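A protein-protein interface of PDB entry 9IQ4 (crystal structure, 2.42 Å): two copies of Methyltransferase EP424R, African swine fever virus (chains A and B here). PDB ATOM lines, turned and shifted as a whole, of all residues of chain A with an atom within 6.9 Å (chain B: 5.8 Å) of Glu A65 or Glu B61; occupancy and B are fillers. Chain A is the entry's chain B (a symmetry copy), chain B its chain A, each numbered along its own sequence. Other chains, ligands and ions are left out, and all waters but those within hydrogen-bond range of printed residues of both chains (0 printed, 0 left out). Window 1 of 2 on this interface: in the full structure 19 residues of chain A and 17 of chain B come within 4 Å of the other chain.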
ATOM      1  N   LEU A  58      10.309 -35.632  -7.000  1.00  0.00           N
ATOM      2  CA  LEU A  58      11.500 -34.795  -7.109  1.00  0.00           C
ATOM      3  C   LEU A  58      12.070 -34.827  -8.518  1.00  0.00           C
ATOM      4  O   LEU A  58      12.348 -33.782  -9.114  1.00  0.00           O
ATOM      5  CB  LEU A  58      12.563 -35.249  -6.114  1.00  0.00           C
ATOM      6  CG  LEU A  58      13.859 -34.427  -6.076  1.00  0.00           C
ATOM      7  CD1 LEU A  58      13.626 -32.919  -6.265  1.00  0.00           C
ATOM      8  CD2 LEU A  58      14.656 -34.703  -4.798  1.00  0.00           C
ATOM      9  N   LEU A  59      12.278 -36.029  -9.055  1.00  0.00           N
ATOM     10  CA  LEU A  59      12.880 -36.152 -10.374  1.00  0.00           C
ATOM     11  C   LEU A  59      11.977 -35.557 -11.450  1.00  0.00           C
ATOM     12  O   LEU A  59      12.462 -34.959 -12.416  1.00  0.00           O
ATOM     13  CB  LEU A  59      13.193 -37.617 -10.661  1.00  0.00           C
ATOM     14  CG  LEU A  59      14.107 -37.951 -11.844  1.00  0.00           C
ATOM     15  CD1 LEU A  59      15.487 -37.335 -11.745  1.00  0.00           C
ATOM     16  CD2 LEU A  59      14.236 -39.467 -11.889  1.00  0.00           C
ATOM     17  N   ASN A  60      10.662 -35.703 -11.308  1.00  0.00           N
ATOM     18  CA  ASN A  60       9.786 -35.067 -12.281  1.00  0.00           C
ATOM     19  C   ASN A  60       9.843 -33.554 -12.148  1.00  0.00           C
ATOM     20  O   ASN A  60       9.881 -32.845 -13.156  1.00  0.00           O
ATOM     21  CB  ASN A  60       8.369 -35.596 -12.139  1.00  0.00           C
ATOM     22  CG  ASN A  60       8.255 -37.036 -12.589  1.00  0.00           C
ATOM     23  OD1 ASN A  60       9.024 -37.498 -13.433  1.00  0.00           O
ATOM     24  ND2 ASN A  60       7.309 -37.758 -12.013  1.00  0.00           N
ATOM     25  N   GLU A  61       9.903 -33.048 -10.912  1.00  0.00           N
ATOM     26  CA  GLU A  61      10.175 -31.633 -10.686  1.00  0.00           C
ATOM     27  C   GLU A  61      11.374 -31.170 -11.502  1.00  0.00           C
ATOM     28  O   GLU A  61      11.263 -30.266 -12.336  1.00  0.00           O
ATOM     29  CB  GLU A  61      10.436 -31.370  -9.211  1.00  0.00           C
ATOM     30  CG  GLU A  61       9.247 -31.349  -8.276  1.00  0.00           C
ATOM     31  CD  GLU A  61       9.722 -31.315  -6.825  1.00  0.00           C
ATOM     32  OE1 GLU A  61      10.943 -31.159  -6.593  1.00  0.00           O
ATOM     33  OE2 GLU A  61       8.892 -31.424  -5.910  1.00  0.00           O
ATOM     34  N   VAL A  62      12.535 -31.791 -11.285  1.00  0.00           N
ATOM     35  CA  VAL A  62      13.725 -31.354 -12.012  1.00  0.00           C
ATOM     36  C   VAL A  62      13.558 -31.575 -13.516  1.00  0.00           C
ATOM     37  O   VAL A  62      13.986 -30.746 -14.327  1.00  0.00           O
ATOM     38  CB  VAL A  62      14.986 -32.045 -11.468  1.00  0.00           C
ATOM     39  CG1 VAL A  62      16.186 -31.487 -12.160  1.00  0.00           C
ATOM     40  CG2 VAL A  62      15.122 -31.830  -9.955  1.00  0.00           C
ATOM     41  N   LYS A  63      12.922 -32.680 -13.921  1.00  0.00           N
ATOM     42  CA  LYS A  63      12.675 -32.869 -15.350  1.00  0.00           C
ATOM     43  C   LYS A  63      11.759 -31.778 -15.888  1.00  0.00           C
ATOM     44  O   LYS A  63      11.986 -31.246 -16.980  1.00  0.00           O
ATOM     45  CB  LYS A  63      12.073 -34.245 -15.620  1.00  0.00           C
ATOM     46  CG  LYS A  63      13.108 -35.335 -15.750  1.00  0.00           C
ATOM     47  CD  LYS A  63      12.633 -36.633 -15.153  1.00  0.00           C
ATOM     48  CE  LYS A  63      13.026 -37.813 -16.020  1.00  0.00           C
ATOM     49  NZ  LYS A  63      12.017 -38.900 -15.915  1.00  0.00           N
ATOM     50  N   ALA A  64      10.737 -31.410 -15.111  1.00  0.00           N
ATOM     51  CA  ALA A  64       9.788 -30.382 -15.512  1.00  0.00           C
ATOM     52  C   ALA A  64      10.434 -29.024 -15.745  1.00  0.00           C
ATOM     53  O   ALA A  64       9.783 -28.145 -16.310  1.00  0.00           O
ATOM     54  CB  ALA A  64       8.684 -30.246 -14.454  1.00  0.00           C
ATOM     55  N   GLU A  65      11.685 -28.824 -15.331  1.00  0.00           N
ATOM     56  CA  GLU A  65      12.316 -27.528 -15.532  1.00  0.00           C
ATOM     57  C   GLU A  65      12.498 -27.193 -17.004  1.00  0.00           C
ATOM     58  O   GLU A  65      12.554 -26.009 -17.356  1.00  0.00           O
ATOM     59  CB  GLU A  65      13.657 -27.474 -14.810  1.00  0.00           C
ATOM     60  CG  GLU A  65      13.522 -27.587 -13.305  1.00  0.00           C
ATOM     61  CD  GLU A  65      14.840 -27.450 -12.600  1.00  0.00           C
ATOM     62  OE1 GLU A  65      15.793 -26.938 -13.227  1.00  0.00           O
ATOM     63  OE2 GLU A  65      14.935 -27.879 -11.434  1.00  0.00           O
ATOM     64  N   MET A  66      12.593 -28.192 -17.883  1.00  0.00           N
ATOM     65  CA  MET A  66      12.757 -27.887 -19.300  1.00  0.00           C
ATOM     66  C   MET A  66      11.432 -27.674 -20.033  1.00  0.00           C
ATOM     67  O   MET A  66      11.453 -27.406 -21.238  1.00  0.00           O
ATOM     68  CB  MET A  66      13.569 -28.982 -20.003  1.00  0.00           C
ATOM     69  CG  MET A  66      14.440 -29.799 -19.076  1.00  0.00           C
ATOM     70  SD  MET A  66      15.195 -31.175 -19.946  1.00  0.00           S
ATOM     71  CE  MET A  66      13.857 -32.357 -19.805  1.00  0.00           C
ATOM     72  N   ASP A  67      10.292 -27.740 -19.335  1.00  0.00           N
ATOM     73  CA  ASP A  67       9.001 -27.418 -19.948  1.00  0.00           C
ATOM     74  C   ASP A  67       8.975 -26.070 -20.649  1.00  0.00           C
ATOM     75  O   ASP A  67       8.596 -26.034 -21.828  1.00  0.00           O
ATOM     76  CB  ASP A  67       7.872 -27.455 -18.909  1.00  0.00           C
ATOM     77  CG  ASP A  67       7.615 -28.842 -18.376  1.00  0.00           C
ATOM     78  OD1 ASP A  67       8.090 -29.828 -18.995  1.00  0.00           O
ATOM     79  OD2 ASP A  67       6.941 -28.938 -17.324  1.00  0.00           O
ATOM     80  N   PRO A  68       9.336 -24.941 -20.015  1.00  0.00           N
ATOM     81  CA  PRO A  68       9.199 -23.656 -20.726  1.00  0.00           C
ATOM     82  C   PRO A  68       9.909 -23.673 -22.056  1.00  0.00           C
ATOM     83  O   PRO A  68       9.383 -23.154 -23.048  1.00  0.00           O
ATOM     84  CB  PRO A  68       9.823 -22.644 -19.755  1.00  0.00           C
ATOM     85  CG  PRO A  68       9.735 -23.322 -18.408  1.00  0.00           C
ATOM     86  CD  PRO A  68      10.014 -24.755 -18.719  1.00  0.00           C
ATOM     87  N   LEU A  69      11.076 -24.329 -22.099  1.00  0.00           N
ATOM     88  CA  LEU A  69      11.836 -24.485 -23.332  1.00  0.00           C
ATOM     89  C   LEU A  69      11.095 -25.329 -24.359  1.00  0.00           C
ATOM     90  O   LEU A  69      11.326 -25.175 -25.567  1.00  0.00           O
ATOM     91  CB  LEU A  69      13.195 -25.101 -23.017  1.00  0.00           C
ATOM     92  CG  LEU A  69      14.101 -24.309 -22.074  1.00  0.00           C
ATOM     93  CD1 LEU A  69      15.479 -24.917 -22.105  1.00  0.00           C
ATOM     94  CD2 LEU A  69      14.147 -22.821 -22.446  1.00  0.00           C
ATOM     95  N   ASN A 238       7.665 -36.974 -18.170  1.00  0.00           N
ATOM     96  CA  ASN A 238       7.636 -37.345 -16.762  1.00  0.00           C
ATOM     97  C   ASN A 238       6.689 -38.501 -16.463  1.00  0.00           C
ATOM     98  O   ASN A 238       6.530 -38.869 -15.295  1.00  0.00           O
ATOM     99  CB  ASN A 238       7.288 -36.119 -15.893  1.00  0.00           C
ATOM    100  CG  ASN A 238       8.286 -34.948 -16.081  1.00  0.00           C
ATOM    101  OD1 ASN A 238       9.235 -35.047 -16.875  1.00  0.00           O
ATOM    102  ND2 ASN A 238       8.090 -33.859 -15.328  1.00  0.00           N
ATOM    103  N   ILE A 363      19.899 -35.607 -11.656  1.00  0.00           N
ATOM    104  CA  ILE A 363      19.511 -34.255 -11.271  1.00  0.00           C
ATOM    105  C   ILE A 363      20.684 -33.279 -11.416  1.00  0.00           C
ATOM    106  O   ILE A 363      20.507 -32.149 -11.898  1.00  0.00           O
ATOM    107  CB  ILE A 363      18.924 -34.275  -9.851  1.00  0.00           C
ATOM    108  CG1 ILE A 363      17.480 -34.793  -9.924  1.00  0.00           C
ATOM    109  CG2 ILE A 363      19.038 -32.908  -9.225  1.00  0.00           C
ATOM    110  CD1 ILE A 363      16.851 -35.068  -8.598  1.00  0.00           C
ATOM    111  N   LEU A 366      21.170 -32.886 -15.113  1.00  0.00           N
ATOM    112  CA  LEU A 366      20.071 -32.068 -15.616  1.00  0.00           C
ATOM    113  C   LEU A 366      20.260 -30.609 -15.211  1.00  0.00           C
ATOM    114  O   LEU A 366      20.077 -29.714 -16.039  1.00  0.00           O
ATOM    115  CB  LEU A 366      18.726 -32.595 -15.122  1.00  0.00           C
ATOM    116  CG  LEU A 366      18.069 -33.843 -15.744  1.00  0.00           C
ATOM    117  CD1 LEU A 366      16.721 -34.074 -15.068  1.00  0.00           C
ATOM    118  CD2 LEU A 366      17.901 -33.750 -17.252  1.00  0.00           C
ATOM    119  N   ASN A 367      20.644 -30.347 -13.952  1.00  0.00           N
ATOM    120  CA  ASN A 367      20.901 -28.966 -13.540  1.00  0.00           C
ATOM    121  C   ASN A 367      22.023 -28.365 -14.371  1.00  0.00           C
ATOM    122  O   ASN A 367      21.901 -27.253 -14.902  1.00  0.00           O
ATOM    123  CB  ASN A 367      21.261 -28.886 -12.053  1.00  0.00           C
ATOM    124  CG  ASN A 367      20.059 -29.092 -11.136  1.00  0.00           C
ATOM    125  OD1 ASN A 367      18.905 -28.973 -11.549  1.00  0.00           O
ATOM    126  ND2 ASN A 367      20.334 -29.424  -9.879  1.00  0.00           N
ATOM    127  N   GLY A 369      22.990 -29.304 -17.312  1.00  0.00           N
ATOM    128  CA  GLY A 369      22.420 -29.069 -18.633  1.00  0.00           C
ATOM    129  C   GLY A 369      21.601 -27.792 -18.718  1.00  0.00           C
ATOM    130  O   GLY A 369      21.701 -27.048 -19.695  1.00  0.00           O
ATOM    131  N   MET A 370      20.780 -27.517 -17.702  1.00  0.00           N
ATOM    132  CA  MET A 370      20.080 -26.231 -17.662  1.00  0.00           C
ATOM    133  C   MET A 370      21.060 -25.060 -17.637  1.00  0.00           C
ATOM    134  O   MET A 370      20.899 -24.085 -18.379  1.00  0.00           O
ATOM    135  CB  MET A 370      19.147 -26.144 -16.449  1.00  0.00           C
ATOM    136  CG  MET A 370      17.851 -26.918 -16.529  1.00  0.00           C
ATOM    137  SD  MET A 370      17.340 -27.516 -18.136  1.00  0.00           S
ATOM    138  CE  MET A 370      17.078 -26.022 -19.107  1.00  0.00           C
ATOM    139  N   LYS A 371      22.062 -25.124 -16.760  1.00  0.00           N
ATOM    140  CA  LYS A 371      23.038 -24.053 -16.706  1.00  0.00           C
ATOM    141  C   LYS A 371      23.737 -23.880 -18.057  1.00  0.00           C
ATOM    142  O   LYS A 371      24.011 -22.750 -18.481  1.00  0.00           O
ATOM    143  CB  LYS A 371      24.046 -24.313 -15.582  1.00  0.00           C
ATOM    144  CG  LYS A 371      24.618 -23.025 -14.985  1.00  0.00           C
ATOM    145  CD  LYS A 371      25.523 -23.276 -13.795  1.00  0.00           C
ATOM    146  CE  LYS A 371      25.965 -21.951 -13.154  1.00  0.00           C
ATOM    147  NZ  LYS A 371      24.819 -21.071 -12.696  1.00  0.00           N
ATOM    148  N   TYR A 373      22.273 -24.649 -21.002  1.00  0.00           N
ATOM    149  CA  TYR A 373      21.265 -23.989 -21.822  1.00  0.00           C
ATOM    150  C   TYR A 373      21.201 -22.504 -21.506  1.00  0.00           C
ATOM    151  O   TYR A 373      21.198 -21.680 -22.413  1.00  0.00           O
ATOM    152  CB  TYR A 373      19.872 -24.609 -21.665  1.00  0.00           C
ATOM    153  CG  TYR A 373      18.877 -23.875 -22.569  1.00  0.00           C
ATOM    154  CD1 TYR A 373      18.300 -22.659 -22.175  1.00  0.00           C
ATOM    155  CD2 TYR A 373      18.567 -24.357 -23.840  1.00  0.00           C
ATOM    156  CE1 TYR A 373      17.450 -21.954 -23.002  1.00  0.00           C
ATOM    157  CE2 TYR A 373      17.692 -23.657 -24.673  1.00  0.00           C
ATOM    158  CZ  TYR A 373      17.137 -22.456 -24.245  1.00  0.00           C
ATOM    159  OH  TYR A 373      16.280 -21.753 -25.052  1.00  0.00           O
ATOM    160  N   ARG A 374      21.119 -22.144 -20.225  1.00  0.00           N
ATOM    161  CA  ARG A 374      20.953 -20.733 -19.865  1.00  0.00           C
ATOM    162  C   ARG A 374      22.064 -19.873 -20.465  1.00  0.00           C
ATOM    163  O   ARG A 374      21.793 -18.838 -21.079  1.00  0.00           O
ATOM    164  CB  ARG A 374      20.918 -20.568 -18.342  1.00  0.00           C
ATOM    165  CG  ARG A 374      19.590 -20.975 -17.698  1.00  0.00           C
ATOM    166  CD  ARG A 374      19.405 -20.337 -16.326  1.00  0.00           C
ATOM    167  NE  ARG A 374      20.452 -20.700 -15.373  1.00  0.00           N
ATOM    168  CZ  ARG A 374      20.548 -21.883 -14.778  1.00  0.00           C
ATOM    169  NH1 ARG A 374      19.673 -22.853 -15.011  1.00  0.00           N
ATOM    170  NH2 ARG A 374      21.543 -22.098 -13.926  1.00  0.00           N
ATOM    171  N   ASP B  56      15.313 -14.904 -16.244  1.00  0.00           N
ATOM    172  CA  ASP B  56      13.974 -15.297 -16.669  1.00  0.00           C
ATOM    173  C   ASP B  56      13.902 -16.793 -16.957  1.00  0.00           C
ATOM    174  O   ASP B  56      12.955 -17.470 -16.537  1.00  0.00           O
ATOM    175  CB  ASP B  56      13.556 -14.489 -17.904  1.00  0.00           C
ATOM    176  CG  ASP B  56      12.057 -14.404 -18.054  1.00  0.00           C
ATOM    177  OD1 ASP B  56      11.412 -13.653 -17.281  1.00  0.00           O
ATOM    178  OD2 ASP B  56      11.503 -15.086 -18.932  1.00  0.00           O
ATOM    179  N   ILE B  57      14.886 -17.322 -17.697  1.00  0.00           N
ATOM    180  CA  ILE B  57      14.912 -18.752 -17.995  1.00  0.00           C
ATOM    181  C   ILE B  57      14.981 -19.561 -16.708  1.00  0.00           C
ATOM    182  O   ILE B  57      14.294 -20.577 -16.554  1.00  0.00           O
ATOM    183  CB  ILE B  57      16.103 -19.102 -18.911  1.00  0.00           C
ATOM    184  CG1 ILE B  57      15.992 -18.466 -20.284  1.00  0.00           C
ATOM    185  CG2 ILE B  57      16.208 -20.625 -19.089  1.00  0.00           C
ATOM    186  CD1 ILE B  57      17.254 -18.619 -21.062  1.00  0.00           C
ATOM    187  N   LEU B  58      15.839 -19.145 -15.777  1.00  0.00           N
ATOM    188  CA  LEU B  58      15.994 -19.889 -14.533  1.00  0.00           C
ATOM    189  C   LEU B  58      14.717 -19.826 -13.699  1.00  0.00           C
ATOM    190  O   LEU B  58      14.196 -20.860 -13.246  1.00  0.00           O
ATOM    191  CB  LEU B  58      17.186 -19.333 -13.753  1.00  0.00           C
ATOM    192  CG  LEU B  58      17.399 -19.854 -12.332  1.00  0.00           C
ATOM    193  CD1 LEU B  58      17.439 -21.380 -12.325  1.00  0.00           C
ATOM    194  CD2 LEU B  58      18.695 -19.272 -11.799  1.00  0.00           C
ATOM    195  N   LEU B  59      14.195 -18.613 -13.499  1.00  0.00           N
ATOM    196  CA  LEU B  59      12.984 -18.443 -12.706  1.00  0.00           C
ATOM    197  C   LEU B  59      11.828 -19.249 -13.290  1.00  0.00           C
ATOM    198  O   LEU B  59      11.024 -19.828 -12.554  1.00  0.00           O
ATOM    199  CB  LEU B  59      12.634 -16.955 -12.617  1.00  0.00           C
ATOM    200  CG  LEU B  59      11.491 -16.620 -11.677  1.00  0.00           C
ATOM    201  CD1 LEU B  59      11.761 -17.249 -10.319  1.00  0.00           C
ATOM    202  CD2 LEU B  59      11.436 -15.143 -11.557  1.00  0.00           C
ATOM    203  N   ASN B  60      11.750 -19.328 -14.611  1.00  0.00           N
ATOM    204  CA  ASN B  60      10.733 -20.178 -15.213  1.00  0.00           C
ATOM    205  C   ASN B  60      11.049 -21.662 -15.061  1.00  0.00           C
ATOM    206  O   ASN B  60      10.123 -22.475 -14.996  1.00  0.00           O
ATOM    207  CB  ASN B  60      10.549 -19.793 -16.677  1.00  0.00           C
ATOM    208  CG  ASN B  60       9.755 -18.516 -16.816  1.00  0.00           C
ATOM    209  OD1 ASN B  60       8.704 -18.370 -16.188  1.00  0.00           O
ATOM    210  ND2 ASN B  60      10.264 -17.571 -17.595  1.00  0.00           N
ATOM    211  N   GLU B  61      12.328 -22.040 -14.995  1.00  0.00           N
ATOM    212  CA  GLU B  61      12.656 -23.439 -14.713  1.00  0.00           C
ATOM    213  C   GLU B  61      12.098 -23.873 -13.363  1.00  0.00           C
ATOM    214  O   GLU B  61      11.481 -24.939 -13.252  1.00  0.00           O
ATOM    215  CB  GLU B  61      14.168 -23.675 -14.738  1.00  0.00           C
ATOM    216  CG  GLU B  61      14.799 -23.530 -16.098  1.00  0.00           C
ATOM    217  CD  GLU B  61      16.317 -23.547 -16.031  1.00  0.00           C
ATOM    218  OE1 GLU B  61      16.863 -23.510 -14.906  1.00  0.00           O
ATOM    219  OE2 GLU B  61      16.963 -23.595 -17.101  1.00  0.00           O
ATOM    220  N   VAL B  62      12.337 -23.067 -12.319  1.00  0.00           N
ATOM    221  CA  VAL B  62      11.894 -23.434 -10.978  1.00  0.00           C
ATOM    222  C   VAL B  62      10.379 -23.389 -10.899  1.00  0.00           C
ATOM    223  O   VAL B  62       9.750 -24.273 -10.304  1.00  0.00           O
ATOM    224  CB  VAL B  62      12.531 -22.522  -9.917  1.00  0.00           C
ATOM    225  CG1 VAL B  62      12.072 -22.951  -8.539  1.00  0.00           C
ATOM    226  CG2 VAL B  62      14.044 -22.562 -10.013  1.00  0.00           C
ATOM    227  N   LYS B  63       9.767 -22.365 -11.497  1.00  0.00           N
ATOM    228  CA  LYS B  63       8.312 -22.346 -11.572  1.00  0.00           C
ATOM    229  C   LYS B  63       7.805 -23.610 -12.241  1.00  0.00           C
ATOM    230  O   LYS B  63       6.857 -24.245 -11.761  1.00  0.00           O
ATOM    231  CB  LYS B  63       7.820 -21.113 -12.328  1.00  0.00           C
ATOM    232  CG  LYS B  63       8.012 -19.807 -11.602  1.00  0.00           C
ATOM    233  CD  LYS B  63       7.486 -18.638 -12.428  1.00  0.00           C
ATOM    234  CE  LYS B  63       7.416 -17.357 -11.592  1.00  0.00           C
ATOM    235  NZ  LYS B  63       7.027 -16.155 -12.401  1.00  0.00           N
ATOM    236  N   ALA B  64       8.449 -24.004 -13.340  1.00  0.00           N
ATOM    237  CA  ALA B  64       8.004 -25.175 -14.074  1.00  0.00           C
ATOM    238  C   ALA B  64       8.004 -26.420 -13.203  1.00  0.00           C
ATOM    239  O   ALA B  64       7.231 -27.345 -13.471  1.00  0.00           O
ATOM    240  CB  ALA B  64       8.887 -25.379 -15.299  1.00  0.00           C
ATOM    241  N   GLU B  65       8.826 -26.447 -12.143  1.00  0.00           N
ATOM    242  CA  GLU B  65       8.941 -27.639 -11.312  1.00  0.00           C
ATOM    243  C   GLU B  65       7.598 -28.127 -10.786  1.00  0.00           C
ATOM    244  O   GLU B  65       7.492 -29.293 -10.383  1.00  0.00           O
ATOM    245  CB  GLU B  65       9.883 -27.372 -10.143  1.00  0.00           C
ATOM    246  CG  GLU B  65      11.355 -27.512 -10.486  1.00  0.00           C
ATOM    247  CD  GLU B  65      12.255 -27.129  -9.327  1.00  0.00           C
ATOM    248  OE1 GLU B  65      11.943 -27.495  -8.174  1.00  0.00           O
ATOM    249  OE2 GLU B  65      13.270 -26.449  -9.566  1.00  0.00           O
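OE2 of Glu A65 sits close to OE2 of Glu B65, 2.9 Å away. The side-chain carboxylate of Glu B61 is in salt-bridge range of the guanidinium group of Arg A374, 2.9 Å away.
The backbone carbonyl oxygen of Asp B56 is in hydrogen-bond range of the side-chain amide nitrogen of Asn B60, at 2.9 Å.
Among the printed residues, merely in contact across the chains: Ala A64 with Ala B64 (3.1 Å), Met A370 with Glu B61 (3.2 Å), Glu A61 with Glu B65 (3.3 Å), Glu A65 with Glu B61 (3.3 Å), Pro A68 with Asn B60 (3.5 Å), Arg A374 with Leu B58 (3.5 Å), Pro A68 with Ala B64 (3.7 Å), Arg A374 with Ile B57 (3.7 Å) and Tyr A373 with Ile B57 (3.9 Å).
Met A66 touches none of the printed residues of chain B. Printed residues of chain B within 4 Å of Tyr A373: Ile B57. Of the printed residues of chain A, Leu B58 touches Arg A374 (3.5 Å). Of chain A, only Glu A65 (3.3 Å), Met A370 (3.2 Å) and Arg A374 (2.9 Å) come within 4 Å of Glu B61. Lys B63 touches none of the printed residues of chain A. The nearest printed residue of chain B that does not touch Pro A68 is Glu B61 (4.5 Å).
Of the 10 printed residues of chain B, 6 touch a printed residue of chain A. Hydrophobic or aromatic side chains of chain B that line the printed part of chain A: Ile B57, Leu B58 and Ala B64. Of the 21 printed residues of chain A, 7 touch a printed residue of chain B. Among the printed residues, Asp or Glu carboxylates within 4 Å of a Lys or Arg side-chain nitrogen of the other chain: Arg A374 with Glu B61.
Glu A61 touches Glu B65, and with the chains exchanged Glu A65 touches Glu B61. Ala B64 touches its own counterpart, Ala A64. Glu A65 touches its own counterpart, Glu B65. 8 positions are printed for both chains. Of the 11 pairs that touch across the chains among the printed residues, 4 have their exchanged pair printed and touching as well.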
